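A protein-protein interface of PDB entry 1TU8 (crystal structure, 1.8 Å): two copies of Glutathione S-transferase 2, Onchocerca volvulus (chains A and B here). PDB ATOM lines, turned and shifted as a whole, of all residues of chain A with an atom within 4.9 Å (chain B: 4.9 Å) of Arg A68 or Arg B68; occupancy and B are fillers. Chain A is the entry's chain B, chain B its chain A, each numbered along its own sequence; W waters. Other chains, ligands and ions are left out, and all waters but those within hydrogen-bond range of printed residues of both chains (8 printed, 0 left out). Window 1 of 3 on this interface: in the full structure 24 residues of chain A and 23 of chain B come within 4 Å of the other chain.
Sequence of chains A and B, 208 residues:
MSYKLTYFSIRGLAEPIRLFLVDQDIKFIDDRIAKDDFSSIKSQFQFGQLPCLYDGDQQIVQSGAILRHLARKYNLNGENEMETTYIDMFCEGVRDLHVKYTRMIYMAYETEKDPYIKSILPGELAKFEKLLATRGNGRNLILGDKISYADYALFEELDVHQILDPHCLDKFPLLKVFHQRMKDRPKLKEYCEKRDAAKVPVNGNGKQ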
ATOM      1  N   GLY A  64     -24.070 -11.478  16.128  1.00  0.00           N
ATOM      2  CA  GLY A  64     -24.053 -12.303  17.330  1.00  0.00           C
ATOM      3  C   GLY A  64     -24.536 -11.561  18.563  1.00  0.00           C
ATOM      4  O   GLY A  64     -25.245 -12.123  19.393  1.00  0.00           O
ATOM      5  N   ALA A  65     -24.160 -10.293  18.688  1.00  0.00           N
ATOM      6  CA  ALA A  65     -24.648  -9.455  19.791  1.00  0.00           C
ATOM      7  C   ALA A  65     -26.142  -9.136  19.666  1.00  0.00           C
ATOM      8  O   ALA A  65     -26.855  -9.105  20.667  1.00  0.00           O
ATOM      9  CB  ALA A  65     -23.827  -8.169  19.889  1.00  0.00           C
ATOM     10  N   ILE A  66     -26.616  -8.924  18.444  1.00  0.00           N
ATOM     11  CA  ILE A  66     -28.039  -8.709  18.196  1.00  0.00           C
ATOM     12  C   ILE A  66     -28.818  -9.937  18.681  1.00  0.00           C
ATOM     13  O   ILE A  66     -29.784  -9.806  19.431  1.00  0.00           O
ATOM     14  CB  ILE A  66     -28.321  -8.425  16.696  1.00  0.00           C
ATOM     15  CG1 ILE A  66     -27.721  -7.077  16.274  1.00  0.00           C
ATOM     16  CG2 ILE A  66     -29.821  -8.405  16.425  1.00  0.00           C
ATOM     17  CD1 ILE A  66     -27.619  -6.890  14.774  1.00  0.00           C
ATOM     18  N   LEU A  67     -28.380 -11.116  18.255  1.00  0.00           N
ATOM     19  CA  LEU A  67     -29.061 -12.374  18.584  1.00  0.00           C
ATOM     20  C   LEU A  67     -29.099 -12.650  20.079  1.00  0.00           C
ATOM     21  O   LEU A  67     -30.134 -13.058  20.635  1.00  0.00           O
ATOM     22  CB  LEU A  67     -28.378 -13.551  17.883  1.00  0.00           C
ATOM     23  CG  LEU A  67     -29.027 -14.166  16.658  1.00  0.00           C
ATOM     24  CD1 LEU A  67     -28.279 -15.456  16.305  1.00  0.00           C
ATOM     25  CD2 LEU A  67     -30.526 -14.447  16.871  1.00  0.00           C
ATOM     26  N   ARG A  68     -27.977 -12.410  20.748  1.00  0.00           N
ATOM     27  CA  ARG A  68     -27.894 -12.670  22.172  1.00  0.00           C
ATOM     28  C   ARG A  68     -28.740 -11.672  22.967  1.00  0.00           C
ATOM     29  O   ARG A  68     -29.333 -12.028  23.990  1.00  0.00           O
ATOM     30  CB  ARG A  68     -26.430 -12.706  22.645  1.00  0.00           C
ATOM     31  CG  ARG A  68     -25.693 -13.978  22.188  1.00  0.00           C
ATOM     32  CD  ARG A  68     -24.252 -14.088  22.684  1.00  0.00           C
ATOM     33  NE  ARG A  68     -23.325 -13.184  21.995  1.00  0.00           N
ATOM     34  CZ  ARG A  68     -22.676 -13.462  20.864  1.00  0.00           C
ATOM     35  NH1 ARG A  68     -22.827 -14.635  20.246  1.00  0.00           N
ATOM     36  NH2 ARG A  68     -21.866 -12.560  20.333  1.00  0.00           N
ATOM     37  N   HIS A  69     -28.833 -10.437  22.473  1.00  0.00           N
ATOM     38  CA  HIS A  69     -29.650  -9.424  23.113  1.00  0.00           C
ATOM     39  C   HIS A  69     -31.136  -9.812  23.026  1.00  0.00           C
ATOM     40  O   HIS A  69     -31.851  -9.793  24.035  1.00  0.00           O
ATOM     41  CB  HIS A  69     -29.399  -8.056  22.478  1.00  0.00           C
ATOM     42  CG  HIS A  69     -30.434  -7.041  22.832  1.00  0.00           C
ATOM     43  ND1 HIS A  69     -31.335  -6.551  21.915  1.00  0.00           N
ATOM     44  CD2 HIS A  69     -30.733  -6.450  24.009  1.00  0.00           C
ATOM     45  CE1 HIS A  69     -32.135  -5.688  22.513  1.00  0.00           C
ATOM     46  NE2 HIS A  69     -31.793  -5.608  23.784  1.00  0.00           N
ATOM     47  N   LEU A  70     -31.584 -10.192  21.833  1.00  0.00           N
ATOM     48  CA  LEU A  70     -32.969 -10.622  21.638  1.00  0.00           C
ATOM     49  C   LEU A  70     -33.271 -11.869  22.485  1.00  0.00           C
ATOM     50  O   LEU A  70     -34.346 -11.977  23.075  1.00  0.00           O
ATOM     51  CB  LEU A  70     -33.236 -10.913  20.165  1.00  0.00           C
ATOM     52  CG  LEU A  70     -33.308  -9.670  19.277  1.00  0.00           C
ATOM     53  CD1 LEU A  70     -33.277 -10.082  17.824  1.00  0.00           C
ATOM     54  CD2 LEU A  70     -34.550  -8.842  19.564  1.00  0.00           C
ATOM     55  N   ALA A  71     -32.315 -12.786  22.531  1.00  0.00           N
ATOM     56  CA  ALA A  71     -32.421 -14.027  23.315  1.00  0.00           C
ATOM     57  C   ALA A  71     -32.655 -13.741  24.802  1.00  0.00           C
ATOM     58  O   ALA A  71     -33.532 -14.336  25.431  1.00  0.00           O
ATOM     59  CB  ALA A  71     -31.175 -14.868  23.126  1.00  0.00           C
ATOM     60  N   ARG A  72     -31.876 -12.823  25.366  1.00  0.00           N
ATOM     61  CA  ARG A  72     -32.087 -12.407  26.755  1.00  0.00           C
ATOM     62  C   ARG A  72     -33.460 -11.796  26.961  1.00  0.00           C
ATOM     63  O   ARG A  72     -34.143 -12.140  27.922  1.00  0.00           O
ATOM     64  CB  ARG A  72     -31.003 -11.424  27.215  1.00  0.00           C
ATOM     65  CG  ARG A  72     -29.690 -12.103  27.510  1.00  0.00           C
ATOM     66  CD  ARG A  72     -28.675 -11.205  28.180  1.00  0.00           C
ATOM     67  NE  ARG A  72     -28.272 -10.104  27.301  1.00  0.00           N
ATOM     68  CZ  ARG A  72     -27.298 -10.166  26.394  1.00  0.00           C
ATOM     69  NH1 ARG A  72     -27.037  -9.104  25.648  1.00  0.00           N
ATOM     70  NH2 ARG A  72     -26.584 -11.270  26.213  1.00  0.00           N
ATOM     71  N   ASP A  88     -24.321 -20.983  23.190  1.00  0.00           N
ATOM     72  CA  ASP A  88     -23.330 -20.021  22.686  1.00  0.00           C
ATOM     73  C   ASP A  88     -22.234 -20.758  21.931  1.00  0.00           C
ATOM     74  O   ASP A  88     -21.919 -20.444  20.784  1.00  0.00           O
ATOM     75  CB  ASP A  88     -22.766 -19.232  23.864  1.00  0.00           C
ATOM     76  CG  ASP A  88     -21.877 -18.076  23.454  1.00  0.00           C
ATOM     77  OD1 ASP A  88     -21.614 -17.865  22.249  1.00  0.00           O
ATOM     78  OD2 ASP A  88     -21.418 -17.303  24.322  1.00  0.00           O
ATOM     79  N   GLU A  92     -21.537 -20.519  17.956  1.00  0.00           N
ATOM     80  CA  GLU A  92     -20.232 -20.111  17.457  1.00  0.00           C
ATOM     81  C   GLU A  92     -19.682 -21.140  16.462  1.00  0.00           C
ATOM     82  O   GLU A  92     -19.018 -20.780  15.510  1.00  0.00           O
ATOM     83  CB  GLU A  92     -19.241 -19.893  18.599  1.00  0.00           C
ATOM     84  CG  GLU A  92     -19.539 -18.647  19.418  1.00  0.00           C
ATOM     85  CD  GLU A  92     -19.299 -17.382  18.622  1.00  0.00           C
ATOM     86  OE1 GLU A  92     -18.121 -17.117  18.282  1.00  0.00           O
ATOM     87  OE2 GLU A  92     -20.283 -16.667  18.316  1.00  0.00           O
ATOM     88  N   TYR A 149     -31.909 -19.289  20.672  1.00  0.00           N
ATOM     89  CA  TYR A 149     -31.489 -18.537  19.493  1.00  0.00           C
ATOM     90  C   TYR A 149     -30.607 -19.361  18.560  1.00  0.00           C
ATOM     91  O   TYR A 149     -30.618 -19.146  17.353  1.00  0.00           O
ATOM     92  CB  TYR A 149     -30.780 -17.237  19.877  1.00  0.00           C
ATOM     93  CG  TYR A 149     -29.408 -17.381  20.520  1.00  0.00           C
ATOM     94  CD1 TYR A 149     -28.249 -17.391  19.749  1.00  0.00           C
ATOM     95  CD2 TYR A 149     -29.271 -17.451  21.903  1.00  0.00           C
ATOM     96  CE1 TYR A 149     -26.989 -17.497  20.333  1.00  0.00           C
ATOM     97  CE2 TYR A 149     -28.017 -17.550  22.498  1.00  0.00           C
ATOM     98  CZ  TYR A 149     -26.878 -17.571  21.710  1.00  0.00           C
ATOM     99  OH  TYR A 149     -25.648 -17.660  22.328  1.00  0.00           O
ATOM    100  N   GLY B  64     -14.962 -17.228  22.032  1.00  0.00           N
ATOM    101  CA  GLY B  64     -15.971 -16.247  22.414  1.00  0.00           C
ATOM    102  C   GLY B  64     -16.930 -16.764  23.471  1.00  0.00           C
ATOM    103  O   GLY B  64     -17.321 -16.019  24.368  1.00  0.00           O
ATOM    104  N   ALA B  65     -17.332 -18.031  23.358  1.00  0.00           N
ATOM    105  CA  ALA B  65     -18.207 -18.649  24.358  1.00  0.00           C
ATOM    106  C   ALA B  65     -17.477 -18.813  25.686  1.00  0.00           C
ATOM    107  O   ALA B  65     -18.058 -18.618  26.744  1.00  0.00           O
ATOM    108  CB  ALA B  65     -18.741 -20.008  23.863  1.00  0.00           C
ATOM    109  N   ILE B  66     -16.198 -19.160  25.625  1.00  0.00           N
ATOM    110  CA  ILE B  66     -15.377 -19.285  26.822  1.00  0.00           C
ATOM    111  C   ILE B  66     -15.318 -17.949  27.568  1.00  0.00           C
ATOM    112  O   ILE B  66     -15.544 -17.888  28.778  1.00  0.00           O
ATOM    113  CB  ILE B  66     -13.951 -19.749  26.451  1.00  0.00           C
ATOM    114  CG1 ILE B  66     -13.973 -21.205  25.961  1.00  0.00           C
ATOM    115  CG2 ILE B  66     -13.011 -19.620  27.634  1.00  0.00           C
ATOM    116  CD1 ILE B  66     -12.726 -21.627  25.257  1.00  0.00           C
ATOM    117  N   LEU B  67     -14.996 -16.885  26.849  1.00  0.00           N
ATOM    118  CA  LEU B  67     -14.806 -15.589  27.493  1.00  0.00           C
ATOM    119  C   LEU B  67     -16.125 -15.051  28.041  1.00  0.00           C
ATOM    120  O   LEU B  67     -16.155 -14.473  29.121  1.00  0.00           O
ATOM    121  CB  LEU B  67     -14.159 -14.592  26.533  1.00  0.00           C
ATOM    122  CG  LEU B  67     -13.622 -13.305  27.160  1.00  0.00           C
ATOM    123  CD1 LEU B  67     -12.522 -13.587  28.166  1.00  0.00           C
ATOM    124  CD2 LEU B  67     -13.130 -12.377  26.069  1.00  0.00           C
ATOM    125  N   ARG B  68     -17.220 -15.264  27.316  1.00  0.00           N
ATOM    126  CA  ARG B  68     -18.542 -14.828  27.778  1.00  0.00           C
ATOM    127  C   ARG B  68     -19.011 -15.593  29.032  1.00  0.00           C
ATOM    128  O   ARG B  68     -19.642 -15.013  29.918  1.00  0.00           O
ATOM    129  CB  ARG B  68     -19.572 -14.933  26.648  1.00  0.00           C
ATOM    130  CG  ARG B  68     -19.504 -13.794  25.658  1.00  0.00           C
ATOM    131  CD  ARG B  68     -20.620 -13.798  24.620  1.00  0.00           C
ATOM    132  NE  ARG B  68     -20.469 -14.860  23.627  1.00  0.00           N
ATOM    133  CZ  ARG B  68     -19.701 -14.775  22.545  1.00  0.00           C
ATOM    134  NH1 ARG B  68     -19.022 -13.662  22.273  1.00  0.00           N
ATOM    135  NH2 ARG B  68     -19.633 -15.802  21.706  1.00  0.00           N
ATOM    136  N   HIS B  69     -18.685 -16.884  29.104  1.00  0.00           N
ATOM    137  CA  HIS B  69     -18.987 -17.715  30.276  1.00  0.00           C
ATOM    138  C   HIS B  69     -18.210 -17.227  31.507  1.00  0.00           C
ATOM    139  O   HIS B  69     -18.786 -17.062  32.586  1.00  0.00           O
ATOM    140  CB  HIS B  69     -18.736 -19.209  29.976  1.00  0.00           C
ATOM    141  CG  HIS B  69     -18.534 -20.045  31.201  1.00  0.00           C
ATOM    142  ND1 HIS B  69     -19.436 -20.068  32.244  1.00  0.00           N
ATOM    143  CD2 HIS B  69     -17.528 -20.877  31.557  1.00  0.00           C
ATOM    144  CE1 HIS B  69     -18.986 -20.865  33.196  1.00  0.00           C
ATOM    145  NE2 HIS B  69     -17.831 -21.371  32.803  1.00  0.00           N
ATOM    146  N   LEU B  70     -16.919 -16.966  31.344  1.00  0.00           N
ATOM    147  CA  LEU B  70     -16.100 -16.433  32.436  1.00  0.00           C
ATOM    148  C   LEU B  70     -16.610 -15.069  32.898  1.00  0.00           C
ATOM    149  O   LEU B  70     -16.684 -14.801  34.083  1.00  0.00           O
ATOM    150  CB  LEU B  70     -14.639 -16.313  32.005  1.00  0.00           C
ATOM    151  CG  LEU B  70     -13.900 -17.641  31.826  1.00  0.00           C
ATOM    152  CD1 LEU B  70     -12.543 -17.381  31.239  1.00  0.00           C
ATOM    153  CD2 LEU B  70     -13.788 -18.402  33.154  1.00  0.00           C
ATOM    154  N   ALA B  71     -16.976 -14.215  31.953  1.00  0.00           N
ATOM    155  CA  ALA B  71     -17.537 -12.912  32.277  1.00  0.00           C
ATOM    156  C   ALA B  71     -18.808 -13.028  33.146  1.00  0.00           C
ATOM    157  O   ALA B  71     -18.981 -12.274  34.095  1.00  0.00           O
ATOM    158  CB  ALA B  71     -17.847 -12.144  30.988  1.00  0.00           C
ATOM    159  N   ARG B  72     -19.696 -13.960  32.816  1.00  0.00           N
ATOM    160  CA  ARG B  72     -20.906 -14.166  33.615  1.00  0.00           C
ATOM    161  C   ARG B  72     -20.536 -14.653  35.005  1.00  0.00           C
ATOM    162  O   ARG B  72     -21.036 -14.161  36.011  1.00  0.00           O
ATOM    163  CB  ARG B  72     -21.827 -15.195  32.969  1.00  0.00           C
ATOM    164  CG  ARG B  72     -22.631 -14.658  31.821  1.00  0.00           C
ATOM    165  CD  ARG B  72     -23.693 -15.622  31.354  1.00  0.00           C
ATOM    166  NE  ARG B  72     -23.140 -16.853  30.799  1.00  0.00           N
ATOM    167  CZ  ARG B  72     -22.728 -17.001  29.541  1.00  0.00           C
ATOM    168  NH1 ARG B  72     -22.802 -16.003  28.675  1.00  0.00           N
ATOM    169  NH2 ARG B  72     -22.256 -18.170  29.141  1.00  0.00           N
ATOM    170  N   ASP B  88     -20.643  -6.812  24.307  1.00  0.00           N
ATOM    171  CA  ASP B  88     -20.732  -7.895  23.334  1.00  0.00           C
ATOM    172  C   ASP B  88     -20.459  -7.343  21.922  1.00  0.00           C
ATOM    173  O   ASP B  88     -19.581  -7.830  21.198  1.00  0.00           O
ATOM    174  CB  ASP B  88     -22.123  -8.536  23.432  1.00  0.00           C
ATOM    175  CG  ASP B  88     -22.212  -9.882  22.759  1.00  0.00           C
ATOM    176  OD1 ASP B  88     -21.258 -10.283  22.068  1.00  0.00           O
ATOM    177  OD2 ASP B  88     -23.226 -10.603  22.879  1.00  0.00           O
ATOM    178  N   GLU B  92     -17.230  -8.208  19.688  1.00  0.00           N
ATOM    179  CA  GLU B  92     -17.392  -8.781  18.357  1.00  0.00           C
ATOM    180  C   GLU B  92     -16.670  -7.943  17.293  1.00  0.00           C
ATOM    181  O   GLU B  92     -16.097  -8.491  16.353  1.00  0.00           O
ATOM    182  CB  GLU B  92     -18.860  -8.956  17.993  1.00  0.00           C
ATOM    183  CG  GLU B  92     -19.564 -10.038  18.784  1.00  0.00           C
ATOM    184  CD  GLU B  92     -19.103 -11.430  18.404  1.00  0.00           C
ATOM    185  OE1 GLU B  92     -18.362 -12.026  19.207  1.00  0.00           O
ATOM    186  OE2 GLU B  92     -19.484 -11.929  17.312  1.00  0.00           O
ATOM    187  N   TYR B 149     -15.013  -8.045  30.293  1.00  0.00           N
ATOM    188  CA  TYR B 149     -14.241  -8.988  29.495  1.00  0.00           C
ATOM    189  C   TYR B 149     -13.748  -8.361  28.192  1.00  0.00           C
ATOM    190  O   TYR B 149     -12.667  -8.696  27.714  1.00  0.00           O
ATOM    191  CB  TYR B 149     -15.028 -10.266  29.241  1.00  0.00           C
ATOM    192  CG  TYR B 149     -16.187 -10.155  28.267  1.00  0.00           C
ATOM    193  CD1 TYR B 149     -16.001 -10.382  26.904  1.00  0.00           C
ATOM    194  CD2 TYR B 149     -17.465  -9.857  28.715  1.00  0.00           C
ATOM    195  CE1 TYR B 149     -17.071 -10.307  26.006  1.00  0.00           C
ATOM    196  CE2 TYR B 149     -18.532  -9.781  27.843  1.00  0.00           C
ATOM    197  CZ  TYR B 149     -18.334 -10.006  26.488  1.00  0.00           C
ATOM    198  OH  TYR B 149     -19.409  -9.944  25.637  1.00  0.00           O
HETATM  199  O   HOH W   1     -21.262 -10.705  15.710  1.00  0.00           O
HETATM  200  O   HOH W   2     -20.944 -14.152  17.849  1.00  0.00           O
HETATM  201  O   HOH W   3     -23.700 -11.088  25.486  1.00  0.00           O
HETATM  202  O   HOH W   4     -20.792 -18.540  26.737  1.00  0.00           O
HETATM  203  O   HOH W   5     -17.702 -14.704  19.533  1.00  0.00           O
HETATM  204  O   HOH W   6     -16.058 -18.290  19.516  1.00  0.00           O
HETATM  205  O   HOH W   7     -23.418 -16.166  25.796  1.00  0.00           O
HETATM  206  O   HOH W   8     -25.554  -8.941  23.143  1.00  0.00           O
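Water W2 lies within hydrogen-bond range of OE2 of Glu A92 (2.6 Å), OE2 of Glu B92 (2.7 Å) and NH1 of Arg A68 (3.1 Å). Water W6 lies within hydrogen-bond range of the side-chain carboxylate of Glu A92 (2.7 Å) and the backbone NH of Gly B64 (2.9 Å). Water W1 bridges OE2 of Glu B92 (2.7 Å) and N of Gly A64 (2.9 Å). Water W3 lies within hydrogen-bond range of the side-chain carboxylate (OD2) of Asp B88 (2.7 Å) and the guanidinium group (NH2) of Arg A72 (3.0 Å). Water W5 lies within hydrogen-bond range of the side-chain carboxylate of Glu A92 (2.8 Å), the side-chain carboxylate of Glu B92 (2.8 Å) and the guanidinium group of Arg B68 (3.1 Å). Water W8 lies within hydrogen-bond range of O of Ala A65 (2.8 Å), OD2 of Asp B88 (2.9 Å) and NH1 of Arg A72 (2.9 Å).
Of the printed residues of chain B, Ala A65 touches Asp B88. Of the printed residues of chain B, Arg A68 touches Arg B68, Asp B88 and Glu B92. Of the printed residues of chain B, Asp A88 touches Ala B65 and Arg B68. Printed residues of chain B within 4 Å of Glu A92: Arg B68. Arg B68 touches three residues of chain A. Printed residues of chain A within 4 Å of Asp B88: Ala A65 (3.6 Å) and Arg A68 (2.7 Å). Printed residues of chain A within 4 Å of Glu B92: Arg A68. The nearest printed residue of chain A that does not touch Arg B68 is Tyr A149 (6.0 Å).
Hydrophobic or aromatic side chains of chain B that line the printed part of chain A: Ala B65. Hydrophobic or aromatic side chains of chain A that line the printed part of chain B: Ala A65. Among the printed residues, Asp or Glu carboxylates within 4 Å of a Lys or Arg side-chain nitrogen of the other chain: Arg A68 with Asp B88 (2.7 Å), Arg A68 with Glu B92 (3.7 Å), Asp A88 with Arg B68 (2.7 Å) and Glu A92 with Arg B68 (3.6 Å).
NH1 of Arg A68 lies within salt-bridge range of OD1 of Asp A88, at 3.99 Å. The guanidinium group (NH1) of Arg B68 is in salt-bridge range of the side-chain carboxylate (OE1) of Glu B92. The backbone carbonyl oxygen (O) of Gly B64 sits close to the guanidinium group (NE) of Arg B68. The backbone carbonyl oxygen (O) of Gly A64 sits close to the guanidinium group (NE) of Arg A68 (3.4 Å). The guanidinium group (NH1) of Arg A68 is in salt-bridge range of the side-chain carboxylate (OE2) of Glu A92, 3.8 Å away.
NE of Arg B68 is in salt-bridge range of OD2 of Asp A88. OE1 of Glu B92 is in salt-bridge range of NH2 of Arg A68, at 3.7 Å. OE2 of Glu A92 is in salt-bridge range of NH2 of Arg B68 (3.6 Å). OD2 of Asp B88 lies within salt-bridge range of NE of Arg A68, at 2.7 Å.
Asp B88 touches Ala A65. Arg A68 touches Arg B68. OD2 of Asp A88 touches CA of Ala B65, 3.5 Å away.
Ala A65 touches Asp B88, and with the chains exchanged Asp A88 touches Ala B65. Arg B68 touches its own counterpart, Arg A68. Arg A68 touches Asp B88, and with the chains exchanged Asp A88 touches Arg B68. Arg A68 touches Glu B92, and with the chains exchanged Glu A92 touches Arg B68. Positions printed for both chains: 64, 65, 66, 67, 68, 69, 70, 71, 72, 88, 92 and 149. Of the 7 pairs that touch across the chains among the printed residues, 7 have their exchanged pair printed and touching as well.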
